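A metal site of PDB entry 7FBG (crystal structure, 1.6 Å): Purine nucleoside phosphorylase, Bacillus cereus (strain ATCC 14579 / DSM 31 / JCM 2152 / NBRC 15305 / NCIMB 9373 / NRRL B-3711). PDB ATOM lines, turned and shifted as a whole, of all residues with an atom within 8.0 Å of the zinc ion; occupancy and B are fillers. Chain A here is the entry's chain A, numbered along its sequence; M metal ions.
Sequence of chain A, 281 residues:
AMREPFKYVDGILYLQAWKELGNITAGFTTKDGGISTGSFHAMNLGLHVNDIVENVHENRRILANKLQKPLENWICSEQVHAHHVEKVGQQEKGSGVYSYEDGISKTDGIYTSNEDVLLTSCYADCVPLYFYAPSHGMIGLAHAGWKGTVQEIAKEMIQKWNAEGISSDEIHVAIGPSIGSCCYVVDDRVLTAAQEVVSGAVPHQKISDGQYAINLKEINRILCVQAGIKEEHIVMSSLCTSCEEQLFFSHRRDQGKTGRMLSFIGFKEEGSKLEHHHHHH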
ATOM      1  N   SER A 178      24.530 -10.391  -6.426  1.00  0.00           N
ATOM      2  CA  SER A 178      25.946 -10.024  -6.207  1.00  0.00           C
ATOM      3  C   SER A 178      26.797 -10.921  -7.089  1.00  0.00           C
ATOM      4  O   SER A 178      26.242 -11.805  -7.719  1.00  0.00           O
ATOM      5  CB  SER A 178      26.347 -10.240  -4.766  1.00  0.00           C
ATOM      6  OG  SER A 178      26.766 -11.568  -4.539  1.00  0.00           O
ATOM      7  N   ILE A 179      28.109 -10.663  -7.107  1.00  0.00           N
ATOM      8  CA  ILE A 179      29.015 -11.557  -7.885  1.00  0.00           C
ATOM      9  C   ILE A 179      29.092 -12.909  -7.177  1.00  0.00           C
ATOM     10  O   ILE A 179      29.277 -12.933  -5.979  1.00  0.00           O
ATOM     11  CB  ILE A 179      30.383 -10.888  -8.163  1.00  0.00           C
ATOM     12  CG1 ILE A 179      31.146 -11.645  -9.250  1.00  0.00           C
ATOM     13  CG2 ILE A 179      31.204 -10.679  -6.901  1.00  0.00           C
ATOM     14  CD1 ILE A 179      32.337 -10.913  -9.776  1.00  0.00           C
ATOM     15  N   GLY A 180      28.856 -13.978  -7.921  1.00  0.00           N
ATOM     16  CA  GLY A 180      28.834 -15.313  -7.320  1.00  0.00           C
ATOM     17  C   GLY A 180      30.181 -15.990  -7.396  1.00  0.00           C
ATOM     18  O   GLY A 180      31.072 -15.425  -7.986  1.00  0.00           O
ATOM     19  N   SER A 181      30.297 -17.203  -6.840  1.00  0.00           N
ATOM     20  CA  SER A 181      31.579 -17.947  -6.774  1.00  0.00           C
ATOM     21  C   SER A 181      31.946 -18.397  -8.184  1.00  0.00           C
ATOM     22  O   SER A 181      33.089 -18.733  -8.410  1.00  0.00           O
ATOM     23  CB  SER A 181      31.448 -19.129  -5.875  1.00  0.00           C
ATOM     24  OG  SER A 181      30.413 -19.996  -6.315  1.00  0.00           O
ATOM     25  N   CYS A 182      30.967 -18.422  -9.060  1.00  0.00           N
ATOM     26  CA  CYS A 182      31.227 -18.756 -10.476  1.00  0.00           C
ATOM     27  C   CYS A 182      32.165 -17.737 -11.095  1.00  0.00           C
ATOM     28  O   CYS A 182      32.913 -18.100 -12.001  1.00  0.00           O
ATOM     29  CB  CYS A 182      29.909 -18.692 -11.221  1.00  0.00           C
ATOM     30  SG  CYS A 182      28.843 -17.360 -10.610  1.00  0.00           S
ATOM     31  N   CYS A 183      32.149 -16.496 -10.593  1.00  0.00           N
ATOM     32  CA  CYS A 183      32.930 -15.418 -11.242  1.00  0.00           C
ATOM     33  C   CYS A 183      33.864 -14.695 -10.277  1.00  0.00           C
ATOM     34  O   CYS A 183      34.680 -13.932 -10.748  1.00  0.00           O
ATOM     35  CB  CYS A 183      32.001 -14.329 -11.752  1.00  0.00           C
ATOM     36  SG  CYS A 183      30.944 -14.944 -13.091  1.00  0.00           S
ATOM     37  N   TYR A 184      33.709 -14.931  -8.987  1.00  0.00           N
ATOM     38  CA  TYR A 184      34.509 -14.138  -8.020  1.00  0.00           C
ATOM     39  C   TYR A 184      35.641 -14.990  -7.435  1.00  0.00           C
ATOM     40  O   TYR A 184      35.381 -15.860  -6.613  1.00  0.00           O
ATOM     41  CB  TYR A 184      33.620 -13.572  -6.921  1.00  0.00           C
ATOM     42  CG  TYR A 184      34.268 -12.545  -6.030  1.00  0.00           C
ATOM     43  CD1 TYR A 184      35.056 -11.525  -6.548  1.00  0.00           C
ATOM     44  CD2 TYR A 184      34.081 -12.582  -4.664  1.00  0.00           C
ATOM     45  CE1 TYR A 184      35.640 -10.587  -5.720  1.00  0.00           C
ATOM     46  CE2 TYR A 184      34.660 -11.651  -3.830  1.00  0.00           C
ATOM     47  CZ  TYR A 184      35.438 -10.647  -4.360  1.00  0.00           C
ATOM     48  OH  TYR A 184      36.006  -9.735  -3.524  1.00  0.00           O
ATOM     49  N   LYS A 217      27.761 -14.031  -0.665  1.00  0.00           N
ATOM     50  CA  LYS A 217      26.356 -14.064  -0.154  1.00  0.00           C
ATOM     51  C   LYS A 217      26.287 -15.058   1.009  1.00  0.00           C
ATOM     52  O   LYS A 217      25.725 -14.713   2.043  1.00  0.00           O
ATOM     53  CB  LYS A 217      25.376 -14.545  -1.222  1.00  0.00           C
ATOM     54  CG  LYS A 217      25.079 -13.593  -2.371  1.00  0.00           C
ATOM     55  CD  LYS A 217      24.112 -14.235  -3.335  1.00  0.00           C
ATOM     56  CE  LYS A 217      23.931 -13.481  -4.634  1.00  0.00           C
ATOM     57  NZ  LYS A 217      25.035 -13.753  -5.584  1.00  0.00           N
ATOM     58  N   SER A 238      20.264 -16.087  -5.610  1.00  0.00           N
ATOM     59  CA  SER A 238      21.395 -16.857  -6.176  1.00  0.00           C
ATOM     60  C   SER A 238      21.887 -16.151  -7.450  1.00  0.00           C
ATOM     61  O   SER A 238      22.770 -16.664  -8.110  1.00  0.00           O
ATOM     62  CB  SER A 238      20.962 -18.254  -6.527  1.00  0.00           C
ATOM     63  OG  SER A 238      19.887 -18.231  -7.442  1.00  0.00           O
ATOM     64  N   LEU A 239      21.302 -14.999  -7.749  1.00  0.00           N
ATOM     65  CA  LEU A 239      21.638 -14.298  -9.012  1.00  0.00           C
ATOM     66  C   LEU A 239      23.057 -13.747  -8.962  1.00  0.00           C
ATOM     67  O   LEU A 239      23.454 -13.201  -7.943  1.00  0.00           O
ATOM     68  CB  LEU A 239      20.629 -13.189  -9.283  1.00  0.00           C
ATOM     69  CG  LEU A 239      19.239 -13.651  -9.719  1.00  0.00           C
ATOM     70  CD1 LEU A 239      18.262 -12.489  -9.696  1.00  0.00           C
ATOM     71  CD2 LEU A 239      19.292 -14.277 -11.100  1.00  0.00           C
ATOM     72  N   CYS A 240      23.770 -13.898 -10.081  1.00  0.00           N
ATOM     73  CA  CYS A 240      25.146 -13.399 -10.178  1.00  0.00           C
ATOM     74  C   CYS A 240      25.179 -12.193 -11.116  1.00  0.00           C
ATOM     75  O   CYS A 240      24.730 -12.312 -12.239  1.00  0.00           O
ATOM     76  CB  CYS A 240      26.080 -14.478 -10.729  1.00  0.00           C
ATOM     77  SG  CYS A 240      27.741 -13.835 -11.076  1.00  0.00           S
ATOM     78  N   THR A 241      25.718 -11.085 -10.629  1.00  0.00           N
ATOM     79  CA  THR A 241      25.766  -9.836 -11.415  1.00  0.00           C
ATOM     80  C   THR A 241      26.614  -9.998 -12.682  1.00  0.00           C
ATOM     81  O   THR A 241      26.301  -9.365 -13.678  1.00  0.00           O
ATOM     82  CB  THR A 241      26.306  -8.717 -10.508  1.00  0.00           C
ATOM     83  OG1 THR A 241      27.422  -9.236  -9.809  1.00  0.00           O
ATOM     84  CG2 THR A 241      25.248  -8.217  -9.553  1.00  0.00           C
ATOM     85  N   SER A 242      27.684 -10.769 -12.582  1.00  0.00           N
ATOM     86  CA  SER A 242      28.592 -10.941 -13.741  1.00  0.00           C
ATOM     87  C   SER A 242      27.964 -11.859 -14.785  1.00  0.00           C
ATOM     88  O   SER A 242      28.055 -11.563 -15.956  1.00  0.00           O
ATOM     89  CB  SER A 242      29.930 -11.446 -13.264  1.00  0.00           C
ATOM     90  OG  SER A 242      30.666 -11.998 -14.338  1.00  0.00           O
ATOM     91  N   CYS A 243      27.310 -12.925 -14.351  1.00  0.00           N
ATOM     92  CA  CYS A 243      26.744 -13.898 -15.314  1.00  0.00           C
ATOM     93  C   CYS A 243      25.542 -13.283 -16.031  1.00  0.00           C
ATOM     94  O   CYS A 243      25.325 -13.629 -17.199  1.00  0.00           O
ATOM     95  CB  CYS A 243      26.269 -15.155 -14.587  1.00  0.00           C
ATOM     96  SG  CYS A 243      27.632 -16.260 -14.105  1.00  0.00           S
ATOM     97  N   GLU A 244      24.749 -12.479 -15.320  1.00  0.00           N
ATOM     98  CA  GLU A 244      23.491 -11.962 -15.933  1.00  0.00           C
ATOM     99  C   GLU A 244      23.815 -10.688 -16.709  1.00  0.00           C
ATOM    100  O   GLU A 244      23.509  -9.611 -16.218  1.00  0.00           O
ATOM    101  CB  GLU A 244      22.406 -11.785 -14.877  1.00  0.00           C
ATOM    102  CG  GLU A 244      22.120 -13.025 -14.062  1.00  0.00           C
ATOM    103  CD  GLU A 244      21.451 -14.189 -14.785  1.00  0.00           C
ATOM    104  OE1 GLU A 244      20.999 -14.000 -15.918  1.00  0.00           O
ATOM    105  OE2 GLU A 244      21.374 -15.263 -14.186  1.00  0.00           O
HETATM  106 ZN    ZN M   1      28.530 -15.951 -11.986  1.00  0.00          ZN
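SG of Cys 240 sits close to N of Ser 242 (3.4 Å).
SG of Cys 183 sits at hydrogen-bond distance from OG of Ser 242, at 3.2 Å.
The side-chain sulfur of Cys 240 lies close to the backbone NH of Gly 180 (3.3 Å).
The side-chain sulfur (SG) of Cys 243 sits close to the side-chain sulfur (SG) of Cys 183, at 3.7 Å.
The zinc ion is bound by SG of Cys 182 (2.0 Å), SG of Cys 243 (2.3 Å) and SG of Cys 240 (2.4 Å).
The zinc ion has three donor atoms within binding distance.
Slightly farther from the zinc ion lies SG of Cys 183 (2.8 Å).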
